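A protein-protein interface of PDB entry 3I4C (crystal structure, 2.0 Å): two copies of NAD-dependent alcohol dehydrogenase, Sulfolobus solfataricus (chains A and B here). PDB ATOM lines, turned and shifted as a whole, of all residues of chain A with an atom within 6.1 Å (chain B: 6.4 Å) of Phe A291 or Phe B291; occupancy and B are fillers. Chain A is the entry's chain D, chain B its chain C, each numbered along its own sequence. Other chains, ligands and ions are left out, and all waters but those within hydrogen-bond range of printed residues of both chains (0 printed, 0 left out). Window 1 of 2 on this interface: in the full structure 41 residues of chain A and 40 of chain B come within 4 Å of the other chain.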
ATOM      1  N   LEU A 254     -25.019   6.048  11.865  1.00  0.00           N
ATOM      2  CA  LEU A 254     -24.974   4.824  11.070  1.00  0.00           C
ATOM      3  C   LEU A 254     -24.676   3.580  11.905  1.00  0.00           C
ATOM      4  O   LEU A 254     -25.066   2.477  11.533  1.00  0.00           O
ATOM      5  CB  LEU A 254     -23.939   4.965   9.941  1.00  0.00           C
ATOM      6  CG  LEU A 254     -24.187   6.095   8.931  1.00  0.00           C
ATOM      7  CD1 LEU A 254     -23.090   6.101   7.865  1.00  0.00           C
ATOM      8  CD2 LEU A 254     -25.553   5.906   8.268  1.00  0.00           C
ATOM      9  N   PRO A 258     -29.539   1.932  12.489  1.00  0.00           N
ATOM     10  CA  PRO A 258     -30.032   0.846  11.639  1.00  0.00           C
ATOM     11  C   PRO A 258     -30.594  -0.281  12.522  1.00  0.00           C
ATOM     12  O   PRO A 258     -31.397  -1.096  12.070  1.00  0.00           O
ATOM     13  CB  PRO A 258     -28.791   0.429  10.867  1.00  0.00           C
ATOM     14  CG  PRO A 258     -28.072   1.747  10.683  1.00  0.00           C
ATOM     15  CD  PRO A 258     -28.206   2.386  12.053  1.00  0.00           C
ATOM     16  N   LEU A 261     -34.446  -0.549  12.815  1.00  0.00           N
ATOM     17  CA  LEU A 261     -35.244  -0.975  11.670  1.00  0.00           C
ATOM     18  C   LEU A 261     -36.056  -2.246  11.892  1.00  0.00           C
ATOM     19  O   LEU A 261     -35.570  -3.226  12.459  1.00  0.00           O
ATOM     20  CB  LEU A 261     -34.348  -1.177  10.444  1.00  0.00           C
ATOM     21  CG  LEU A 261     -33.586   0.036   9.905  1.00  0.00           C
ATOM     22  CD1 LEU A 261     -32.438  -0.432   9.018  1.00  0.00           C
ATOM     23  CD2 LEU A 261     -34.535   0.939   9.121  1.00  0.00           C
ATOM     24  N   GLY A 265     -37.434  -2.814   6.723  1.00  0.00           N
ATOM     25  CA  GLY A 265     -37.209  -1.398   6.950  1.00  0.00           C
ATOM     26  C   GLY A 265     -36.223  -0.789   5.961  1.00  0.00           C
ATOM     27  O   GLY A 265     -35.295  -1.463   5.490  1.00  0.00           O
ATOM     28  N   LYS A 266     -36.431   0.490   5.643  1.00  0.00           N
ATOM     29  CA  LYS A 266     -35.570   1.214   4.720  1.00  0.00           C
ATOM     30  C   LYS A 266     -34.780   2.308   5.436  1.00  0.00           C
ATOM     31  O   LYS A 266     -35.359   3.205   6.038  1.00  0.00           O
ATOM     32  CB  LYS A 266     -36.403   1.857   3.602  1.00  0.00           C
ATOM     33  CG  LYS A 266     -37.196   0.853   2.761  1.00  0.00           C
ATOM     34  CD  LYS A 266     -37.654   1.466   1.447  1.00  0.00           C
ATOM     35  CE  LYS A 266     -38.413   0.443   0.621  1.00  0.00           C
ATOM     36  NZ  LYS A 266     -38.511   0.817  -0.826  1.00  0.00           N
ATOM     37  N   TYR A 267     -33.457   2.234   5.367  1.00  0.00           N
ATOM     38  CA  TYR A 267     -32.620   3.240   6.004  1.00  0.00           C
ATOM     39  C   TYR A 267     -32.194   4.226   4.929  1.00  0.00           C
ATOM     40  O   TYR A 267     -31.332   3.923   4.107  1.00  0.00           O
ATOM     41  CB  TYR A 267     -31.390   2.595   6.657  1.00  0.00           C
ATOM     42  CG  TYR A 267     -30.714   3.499   7.678  1.00  0.00           C
ATOM     43  CD1 TYR A 267     -29.872   4.530   7.277  1.00  0.00           C
ATOM     44  CD2 TYR A 267     -30.969   3.352   9.042  1.00  0.00           C
ATOM     45  CE1 TYR A 267     -29.292   5.405   8.221  1.00  0.00           C
ATOM     46  CE2 TYR A 267     -30.408   4.210   9.982  1.00  0.00           C
ATOM     47  CZ  TYR A 267     -29.570   5.237   9.565  1.00  0.00           C
ATOM     48  OH  TYR A 267     -29.037   6.099  10.489  1.00  0.00           O
ATOM     49  N   VAL A 268     -32.824   5.399   4.923  1.00  0.00           N
ATOM     50  CA  VAL A 268     -32.524   6.420   3.924  1.00  0.00           C
ATOM     51  C   VAL A 268     -31.443   7.362   4.444  1.00  0.00           C
ATOM     52  O   VAL A 268     -31.685   8.162   5.356  1.00  0.00           O
ATOM     53  CB  VAL A 268     -33.784   7.245   3.567  1.00  0.00           C
ATOM     54  CG1 VAL A 268     -33.461   8.218   2.452  1.00  0.00           C
ATOM     55  CG2 VAL A 268     -34.926   6.314   3.148  1.00  0.00           C
ATOM     56  N   MET A 269     -30.257   7.248   3.854  1.00  0.00           N
ATOM     57  CA  MET A 269     -29.094   8.053   4.235  1.00  0.00           C
ATOM     58  C   MET A 269     -28.925   9.204   3.262  1.00  0.00           C
ATOM     59  O   MET A 269     -28.979   9.001   2.047  1.00  0.00           O
ATOM     60  CB  MET A 269     -27.814   7.228   4.155  1.00  0.00           C
ATOM     61  CG  MET A 269     -27.771   5.941   4.915  1.00  0.00           C
ATOM     62  SD  MET A 269     -26.470   4.909   4.160  1.00  0.00           S
ATOM     63  CE  MET A 269     -25.158   6.062   4.044  1.00  0.00           C
ATOM     64  N   LEU A 277     -20.497   2.714   5.928  1.00  0.00           N
ATOM     65  CA  LEU A 277     -21.632   1.970   6.431  1.00  0.00           C
ATOM     66  C   LEU A 277     -21.054   0.603   6.783  1.00  0.00           C
ATOM     67  O   LEU A 277     -20.350  -0.010   5.975  1.00  0.00           O
ATOM     68  CB  LEU A 277     -22.710   1.836   5.351  1.00  0.00           C
ATOM     69  CG  LEU A 277     -23.929   0.987   5.733  1.00  0.00           C
ATOM     70  CD1 LEU A 277     -24.619   1.593   6.943  1.00  0.00           C
ATOM     71  CD2 LEU A 277     -24.886   0.898   4.554  1.00  0.00           C
ATOM     72  N   TYR A 279     -22.375  -3.030   8.427  1.00  0.00           N
ATOM     73  CA  TYR A 279     -23.498  -3.804   8.934  1.00  0.00           C
ATOM     74  C   TYR A 279     -23.343  -5.282   8.608  1.00  0.00           C
ATOM     75  O   TYR A 279     -22.890  -5.644   7.522  1.00  0.00           O
ATOM     76  CB  TYR A 279     -24.805  -3.267   8.343  1.00  0.00           C
ATOM     77  CG  TYR A 279     -25.979  -3.371   9.284  1.00  0.00           C
ATOM     78  CD1 TYR A 279     -26.015  -2.625  10.462  1.00  0.00           C
ATOM     79  CD2 TYR A 279     -27.043  -4.230   9.016  1.00  0.00           C
ATOM     80  CE1 TYR A 279     -27.078  -2.735  11.352  1.00  0.00           C
ATOM     81  CE2 TYR A 279     -28.114  -4.346   9.901  1.00  0.00           C
ATOM     82  CZ  TYR A 279     -28.122  -3.596  11.067  1.00  0.00           C
ATOM     83  OH  TYR A 279     -29.177  -3.706  11.954  1.00  0.00           O
ATOM     84  N   ILE A 284     -29.130  -8.216   7.320  1.00  0.00           N
ATOM     85  CA  ILE A 284     -29.778  -7.616   6.168  1.00  0.00           C
ATOM     86  C   ILE A 284     -30.658  -8.618   5.423  1.00  0.00           C
ATOM     87  O   ILE A 284     -31.803  -8.312   5.098  1.00  0.00           O
ATOM     88  CB  ILE A 284     -28.724  -7.042   5.199  1.00  0.00           C
ATOM     89  CG1 ILE A 284     -27.885  -5.984   5.921  1.00  0.00           C
ATOM     90  CG2 ILE A 284     -29.400  -6.426   3.994  1.00  0.00           C
ATOM     91  CD1 ILE A 284     -26.762  -5.417   5.086  1.00  0.00           C
ATOM     92  N   ILE A 289     -33.857  -5.861   5.123  1.00  0.00           N
ATOM     93  CA  ILE A 289     -33.726  -4.416   5.251  1.00  0.00           C
ATOM     94  C   ILE A 289     -33.012  -3.852   4.030  1.00  0.00           C
ATOM     95  O   ILE A 289     -32.397  -4.581   3.254  1.00  0.00           O
ATOM     96  CB  ILE A 289     -32.964  -3.982   6.523  1.00  0.00           C
ATOM     97  CG1 ILE A 289     -31.624  -4.706   6.611  1.00  0.00           C
ATOM     98  CG2 ILE A 289     -33.836  -4.217   7.761  1.00  0.00           C
ATOM     99  CD1 ILE A 289     -30.761  -4.234   7.765  1.00  0.00           C
ATOM    100  N   GLN A 290     -33.111  -2.539   3.869  1.00  0.00           N
ATOM    101  CA  GLN A 290     -32.504  -1.851   2.751  1.00  0.00           C
ATOM    102  C   GLN A 290     -31.820  -0.573   3.196  1.00  0.00           C
ATOM    103  O   GLN A 290     -32.359   0.184   4.014  1.00  0.00           O
ATOM    104  CB  GLN A 290     -33.575  -1.473   1.729  1.00  0.00           C
ATOM    105  CG  GLN A 290     -34.517  -2.593   1.342  1.00  0.00           C
ATOM    106  CD  GLN A 290     -35.623  -2.109   0.421  1.00  0.00           C
ATOM    107  OE1 GLN A 290     -35.362  -1.472  -0.600  1.00  0.00           O
ATOM    108  NE2 GLN A 290     -36.867  -2.404   0.783  1.00  0.00           N
ATOM    109  N   PHE A 291     -30.627  -0.341   2.665  1.00  0.00           N
ATOM    110  CA  PHE A 291     -29.895   0.890   2.928  1.00  0.00           C
ATOM    111  C   PHE A 291     -29.992   1.617   1.584  1.00  0.00           C
ATOM    112  O   PHE A 291     -29.598   1.073   0.550  1.00  0.00           O
ATOM    113  CB  PHE A 291     -28.435   0.594   3.296  1.00  0.00           C
ATOM    114  CG  PHE A 291     -28.268   0.022   4.680  1.00  0.00           C
ATOM    115  CD1 PHE A 291     -28.306   0.852   5.800  1.00  0.00           C
ATOM    116  CD2 PHE A 291     -28.106  -1.344   4.867  1.00  0.00           C
ATOM    117  CE1 PHE A 291     -28.184   0.326   7.093  1.00  0.00           C
ATOM    118  CE2 PHE A 291     -27.985  -1.883   6.152  1.00  0.00           C
ATOM    119  CZ  PHE A 291     -28.025  -1.038   7.271  1.00  0.00           C
ATOM    120  N   VAL A 292     -30.548   2.823   1.585  1.00  0.00           N
ATOM    121  CA  VAL A 292     -30.701   3.559   0.339  1.00  0.00           C
ATOM    122  C   VAL A 292     -30.158   4.982   0.453  1.00  0.00           C
ATOM    123  O   VAL A 292     -30.438   5.703   1.416  1.00  0.00           O
ATOM    124  CB  VAL A 292     -32.195   3.590  -0.123  1.00  0.00           C
ATOM    125  CG1 VAL A 292     -32.880   2.272   0.238  1.00  0.00           C
ATOM    126  CG2 VAL A 292     -32.923   4.749   0.479  1.00  0.00           C
ATOM    127  N   GLY A 293     -29.363   5.373  -0.535  1.00  0.00           N
ATOM    128  CA  GLY A 293     -28.782   6.697  -0.512  1.00  0.00           C
ATOM    129  C   GLY A 293     -29.569   7.681  -1.342  1.00  0.00           C
ATOM    130  O   GLY A 293     -30.325   7.289  -2.231  1.00  0.00           O
ATOM    131  N   LEU B 254     -18.652  -9.198  -1.435  1.00  0.00           N
ATOM    132  CA  LEU B 254     -19.144  -7.928  -0.907  1.00  0.00           C
ATOM    133  C   LEU B 254     -18.115  -6.807  -0.988  1.00  0.00           C
ATOM    134  O   LEU B 254     -18.478  -5.633  -1.026  1.00  0.00           O
ATOM    135  CB  LEU B 254     -19.625  -8.076   0.546  1.00  0.00           C
ATOM    136  CG  LEU B 254     -20.854  -8.953   0.827  1.00  0.00           C
ATOM    137  CD1 LEU B 254     -21.221  -8.858   2.306  1.00  0.00           C
ATOM    138  CD2 LEU B 254     -22.031  -8.510  -0.027  1.00  0.00           C
ATOM    139  N   PRO B 258     -19.767  -4.476  -5.268  1.00  0.00           N
ATOM    140  CA  PRO B 258     -20.550  -3.241  -5.199  1.00  0.00           C
ATOM    141  C   PRO B 258     -19.888  -2.161  -6.062  1.00  0.00           C
ATOM    142  O   PRO B 258     -20.532  -1.201  -6.472  1.00  0.00           O
ATOM    143  CB  PRO B 258     -20.521  -2.892  -3.713  1.00  0.00           C
ATOM    144  CG  PRO B 258     -20.489  -4.247  -3.067  1.00  0.00           C
ATOM    145  CD  PRO B 258     -19.451  -4.971  -3.918  1.00  0.00           C
ATOM    146  N   LEU B 261     -21.542  -1.433  -9.446  1.00  0.00           N
ATOM    147  CA  LEU B 261     -22.860  -0.809  -9.490  1.00  0.00           C
ATOM    148  C   LEU B 261     -22.920   0.512 -10.240  1.00  0.00           C
ATOM    149  O   LEU B 261     -22.041   1.367 -10.109  1.00  0.00           O
ATOM    150  CB  LEU B 261     -23.389  -0.568  -8.075  1.00  0.00           C
ATOM    151  CG  LEU B 261     -23.853  -1.757  -7.233  1.00  0.00           C
ATOM    152  CD1 LEU B 261     -24.135  -1.285  -5.805  1.00  0.00           C
ATOM    153  CD2 LEU B 261     -25.112  -2.363  -7.852  1.00  0.00           C
ATOM    154  N   GLY B 265     -28.006   1.757  -8.775  1.00  0.00           N
ATOM    155  CA  GLY B 265     -27.880   0.309  -8.787  1.00  0.00           C
ATOM    156  C   GLY B 265     -28.342  -0.333  -7.486  1.00  0.00           C
ATOM    157  O   GLY B 265     -28.205   0.248  -6.402  1.00  0.00           O
ATOM    158  N   LYS B 266     -28.906  -1.530  -7.592  1.00  0.00           N
ATOM    159  CA  LYS B 266     -29.386  -2.246  -6.424  1.00  0.00           C
ATOM    160  C   LYS B 266     -28.567  -3.509  -6.230  1.00  0.00           C
ATOM    161  O   LYS B 266     -28.451  -4.343  -7.138  1.00  0.00           O
ATOM    162  CB  LYS B 266     -30.872  -2.593  -6.579  1.00  0.00           C
ATOM    163  CG  LYS B 266     -31.786  -1.371  -6.660  1.00  0.00           C
ATOM    164  CD  LYS B 266     -33.259  -1.768  -6.551  1.00  0.00           C
ATOM    165  CE  LYS B 266     -34.160  -0.536  -6.585  1.00  0.00           C
ATOM    166  NZ  LYS B 266     -35.574  -0.814  -6.155  1.00  0.00           N
ATOM    167  N   TYR B 267     -28.005  -3.639  -5.037  1.00  0.00           N
ATOM    168  CA  TYR B 267     -27.177  -4.779  -4.707  1.00  0.00           C
ATOM    169  C   TYR B 267     -28.015  -5.710  -3.841  1.00  0.00           C
ATOM    170  O   TYR B 267     -28.258  -5.426  -2.667  1.00  0.00           O
ATOM    171  CB  TYR B 267     -25.924  -4.297  -3.967  1.00  0.00           C
ATOM    172  CG  TYR B 267     -24.801  -5.306  -3.960  1.00  0.00           C
ATOM    173  CD1 TYR B 267     -24.808  -6.385  -3.075  1.00  0.00           C
ATOM    174  CD2 TYR B 267     -23.758  -5.219  -4.889  1.00  0.00           C
ATOM    175  CE1 TYR B 267     -23.804  -7.356  -3.119  1.00  0.00           C
ATOM    176  CE2 TYR B 267     -22.759  -6.182  -4.944  1.00  0.00           C
ATOM    177  CZ  TYR B 267     -22.786  -7.250  -4.060  1.00  0.00           C
ATOM    178  OH  TYR B 267     -21.809  -8.228  -4.140  1.00  0.00           O
ATOM    179  N   VAL B 268     -28.484  -6.802  -4.438  1.00  0.00           N
ATOM    180  CA  VAL B 268     -29.304  -7.769  -3.718  1.00  0.00           C
ATOM    181  C   VAL B 268     -28.425  -8.885  -3.167  1.00  0.00           C
ATOM    182  O   VAL B 268     -27.830  -9.662  -3.921  1.00  0.00           O
ATOM    183  CB  VAL B 268     -30.402  -8.380  -4.631  1.00  0.00           C
ATOM    184  CG1 VAL B 268     -31.326  -9.267  -3.814  1.00  0.00           C
ATOM    185  CG2 VAL B 268     -31.207  -7.267  -5.295  1.00  0.00           C
ATOM    186  N   MET B 269     -28.352  -8.945  -1.841  1.00  0.00           N
ATOM    187  CA  MET B 269     -27.548  -9.940  -1.131  1.00  0.00           C
ATOM    188  C   MET B 269     -28.450 -11.064  -0.650  1.00  0.00           C
ATOM    189  O   MET B 269     -29.504 -10.812  -0.068  1.00  0.00           O
ATOM    190  CB  MET B 269     -26.873  -9.291   0.080  1.00  0.00           C
ATOM    191  CG  MET B 269     -26.057  -8.058  -0.249  1.00  0.00           C
ATOM    192  SD  MET B 269     -25.847  -6.988   1.197  1.00  0.00           S
ATOM    193  CE  MET B 269     -25.454  -8.169   2.412  1.00  0.00           C
ATOM    194  N   LEU B 277     -21.010  -6.115   5.694  1.00  0.00           N
ATOM    195  CA  LEU B 277     -21.074  -5.247   4.535  1.00  0.00           C
ATOM    196  C   LEU B 277     -20.310  -4.005   4.952  1.00  0.00           C
ATOM    197  O   LEU B 277     -20.593  -3.431   6.001  1.00  0.00           O
ATOM    198  CB  LEU B 277     -22.525  -4.863   4.214  1.00  0.00           C
ATOM    199  CG  LEU B 277     -22.719  -3.603   3.353  1.00  0.00           C
ATOM    200  CD1 LEU B 277     -22.006  -3.759   2.024  1.00  0.00           C
ATOM    201  CD2 LEU B 277     -24.197  -3.354   3.126  1.00  0.00           C
ATOM    202  N   TYR B 279     -19.029  -0.369   3.253  1.00  0.00           N
ATOM    203  CA  TYR B 279     -19.006   0.517   2.096  1.00  0.00           C
ATOM    204  C   TYR B 279     -19.000   1.986   2.492  1.00  0.00           C
ATOM    205  O   TYR B 279     -19.693   2.388   3.421  1.00  0.00           O
ATOM    206  CB  TYR B 279     -20.214   0.252   1.190  1.00  0.00           C
ATOM    207  CG  TYR B 279     -19.922   0.493  -0.274  1.00  0.00           C
ATOM    208  CD1 TYR B 279     -19.003  -0.306  -0.955  1.00  0.00           C
ATOM    209  CD2 TYR B 279     -20.543   1.525  -0.976  1.00  0.00           C
ATOM    210  CE1 TYR B 279     -18.706  -0.091  -2.296  1.00  0.00           C
ATOM    211  CE2 TYR B 279     -20.252   1.751  -2.330  1.00  0.00           C
ATOM    212  CZ  TYR B 279     -19.328   0.935  -2.979  1.00  0.00           C
ATOM    213  OH  TYR B 279     -19.016   1.135  -4.309  1.00  0.00           O
ATOM    214  N   ILE B 284     -22.601   5.870  -1.469  1.00  0.00           N
ATOM    215  CA  ILE B 284     -23.997   5.438  -1.489  1.00  0.00           C
ATOM    216  C   ILE B 284     -24.947   6.582  -1.802  1.00  0.00           C
ATOM    217  O   ILE B 284     -25.864   6.434  -2.609  1.00  0.00           O
ATOM    218  CB  ILE B 284     -24.405   4.811  -0.147  1.00  0.00           C
ATOM    219  CG1 ILE B 284     -23.501   3.610   0.141  1.00  0.00           C
ATOM    220  CG2 ILE B 284     -25.886   4.388  -0.188  1.00  0.00           C
ATOM    221  CD1 ILE B 284     -23.767   2.944   1.468  1.00  0.00           C
ATOM    222  N   ILE B 289     -27.276   4.397  -4.623  1.00  0.00           N
ATOM    223  CA  ILE B 289     -27.327   2.947  -4.693  1.00  0.00           C
ATOM    224  C   ILE B 289     -28.074   2.386  -3.493  1.00  0.00           C
ATOM    225  O   ILE B 289     -28.334   3.093  -2.516  1.00  0.00           O
ATOM    226  CB  ILE B 289     -25.919   2.307  -4.795  1.00  0.00           C
ATOM    227  CG1 ILE B 289     -25.108   2.590  -3.543  1.00  0.00           C
ATOM    228  CG2 ILE B 289     -25.202   2.828  -6.051  1.00  0.00           C
ATOM    229  CD1 ILE B 289     -23.756   1.887  -3.528  1.00  0.00           C
ATOM    230  N   GLN B 290     -28.453   1.120  -3.586  1.00  0.00           N
ATOM    231  CA  GLN B 290     -29.169   0.471  -2.507  1.00  0.00           C
ATOM    232  C   GLN B 290     -28.600  -0.913  -2.267  1.00  0.00           C
ATOM    233  O   GLN B 290     -28.234  -1.621  -3.212  1.00  0.00           O
ATOM    234  CB  GLN B 290     -30.665   0.333  -2.851  1.00  0.00           C
ATOM    235  CG  GLN B 290     -31.400   1.638  -3.108  1.00  0.00           C
ATOM    236  CD  GLN B 290     -32.875   1.431  -3.439  1.00  0.00           C
ATOM    237  OE1 GLN B 290     -33.554   0.588  -2.842  1.00  0.00           O
ATOM    238  NE2 GLN B 290     -33.382   2.213  -4.384  1.00  0.00           N
ATOM    239  N   PHE B 291     -28.517  -1.288  -0.995  1.00  0.00           N
ATOM    240  CA  PHE B 291     -28.063  -2.615  -0.612  1.00  0.00           C
ATOM    241  C   PHE B 291     -29.329  -3.209  -0.011  1.00  0.00           C
ATOM    242  O   PHE B 291     -29.905  -2.623   0.902  1.00  0.00           O
ATOM    243  CB  PHE B 291     -26.955  -2.510   0.430  1.00  0.00           C
ATOM    244  CG  PHE B 291     -25.666  -1.969  -0.119  1.00  0.00           C
ATOM    245  CD1 PHE B 291     -24.752  -2.814  -0.749  1.00  0.00           C
ATOM    246  CD2 PHE B 291     -25.374  -0.616  -0.031  1.00  0.00           C
ATOM    247  CE1 PHE B 291     -23.563  -2.312  -1.285  1.00  0.00           C
ATOM    248  CE2 PHE B 291     -24.191  -0.105  -0.562  1.00  0.00           C
ATOM    249  CZ  PHE B 291     -23.283  -0.955  -1.191  1.00  0.00           C
ATOM    250  N   VAL B 292     -29.787  -4.339  -0.541  1.00  0.00           N
ATOM    251  CA  VAL B 292     -31.004  -4.957  -0.025  1.00  0.00           C
ATOM    252  C   VAL B 292     -30.826  -6.448   0.198  1.00  0.00           C
ATOM    253  O   VAL B 292     -30.212  -7.143  -0.612  1.00  0.00           O
ATOM    254  CB  VAL B 292     -32.212  -4.721  -0.975  1.00  0.00           C
ATOM    255  CG1 VAL B 292     -32.302  -3.239  -1.340  1.00  0.00           C
ATOM    256  CG2 VAL B 292     -32.084  -5.561  -2.227  1.00  0.00           C
ATOM    257  N   GLY B 293     -31.365  -6.931   1.311  1.00  0.00           N
ATOM    258  CA  GLY B 293     -31.249  -8.340   1.634  1.00  0.00           C
ATOM    259  C   GLY B 293     -32.496  -9.128   1.278  1.00  0.00           C
ATOM    260  O   GLY B 293     -33.599  -8.582   1.209  1.00  0.00           O
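Printed residues of chain A that touch a printed residue of chain B: Leu A277, Tyr A279, Ile A284, Ile A289, Gln A290, Phe A291, Val A292 and Gly A293.
Hydrophobic or aromatic side chains of chain A within 4 Å of the printed part of chain B: Leu A277, Ile A284 and Val A292.
Hydrophobic or aromatic side chains of chain B within 4 Å of the printed part of chain A: Leu B277, Ile B284 and Val B292.
Leu A277 touches Ile B284, and with the chains exchanged Ile A284 touches Leu B277.
Ile A284 touches Gly B293, and with the chains exchanged Gly A293 touches Ile B284.
Gln B290 touches its own counterpart, Gln A290.
Phe B291 touches its own counterpart, Phe A291.
Positions printed for both chains: 254, 258, 261, 265, 266, 267, 268, 269, 277, 279, 284, 289, 290, 291, 292 and 293.
Among the printed residues, pairs that only touch across the chains: Leu A277 with Ile B284 (3.9 Å), Ile A284 with Leu B277 (3.8 Å), Ile A284 with Gly B293 (3.4 Å), Ile A289 with Phe B291 (3.9 Å), Ile A289 with Val B292 (3.6 Å), Gln A290 with Gln B290 (3.5 Å), Gln A290 with Phe B291 (3.3 Å), Gln A290 with Val B292 (3.5 Å), Phe A291 with Ile B289 (3.9 Å), Phe A291 with Gln B290 (3.1 Å), Val A292 with Ile B289 (3.7 Å), Val A292 with Gln B290 (3.6 Å) and Gly A293 with Ile B284 (3.6 Å).
The backbone carbonyl oxygen (O) of Gly B265 lies within hydrogen-bond range of the backbone NH (N) of Gln B290 (3.0 Å).
O of Tyr B267 is in hydrogen-bond range of N of Val B292 (2.8 Å).
O of Val B292 is in hydrogen-bond range of N of Met B269, at 2.9 Å.
The backbone carbonyl oxygen (O) of Ile B284 is in hydrogen-bond range of the backbone NH (N) of Ile B289 (3.2 Å).
The backbone carbonyl oxygen of Gln A290 is in hydrogen-bond range of the backbone NH of Tyr A267 (2.7 Å).
The backbone carbonyl oxygen of Ile A284 sits at hydrogen-bond distance from the backbone NH of Ile A289, 3.2 Å away.
Of chain B, only Ile B289 (3.9 Å), Gln B290 (3.1 Å) and Phe B291 (3.0 Å) come within 4 Å of Phe A291.
Of the printed residues of chain A, Ile B284 touches Leu A277 (3.9 Å) and Gly A293 (3.6 Å).
Of the printed residues of chain B, Gly A293 touches Ile B284 and Ile B289.
Lys B266 touches none of the printed residues of chain A.
The nearest residue of chain A that does not touch Phe B291 is Leu A277 (4.9 Å).
The nearest printed residue of chain A that does not touch Ile B289 is Met A269 (7.2 Å).
The backbone NH (N) of Leu B277 sits at hydrogen-bond distance from the backbone carbonyl oxygen (O) of Tyr A279 (2.7 Å).
O of Tyr B279 sits at hydrogen-bond distance from N of Leu A277 (2.7 Å).
O of Ile B289 sits at hydrogen-bond distance from N of Gly A293 (3.2 Å).
The backbone carbonyl oxygen (O) of Phe B291 is in hydrogen-bond range of the backbone NH (N) of Phe A291, 3.0 Å away.
The backbone carbonyl oxygen (O) of Ile A289 sits at hydrogen-bond distance from the backbone NH (N) of Gly B293 (3.2 Å).
O of Leu A277 lies close to O of Leu B277.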
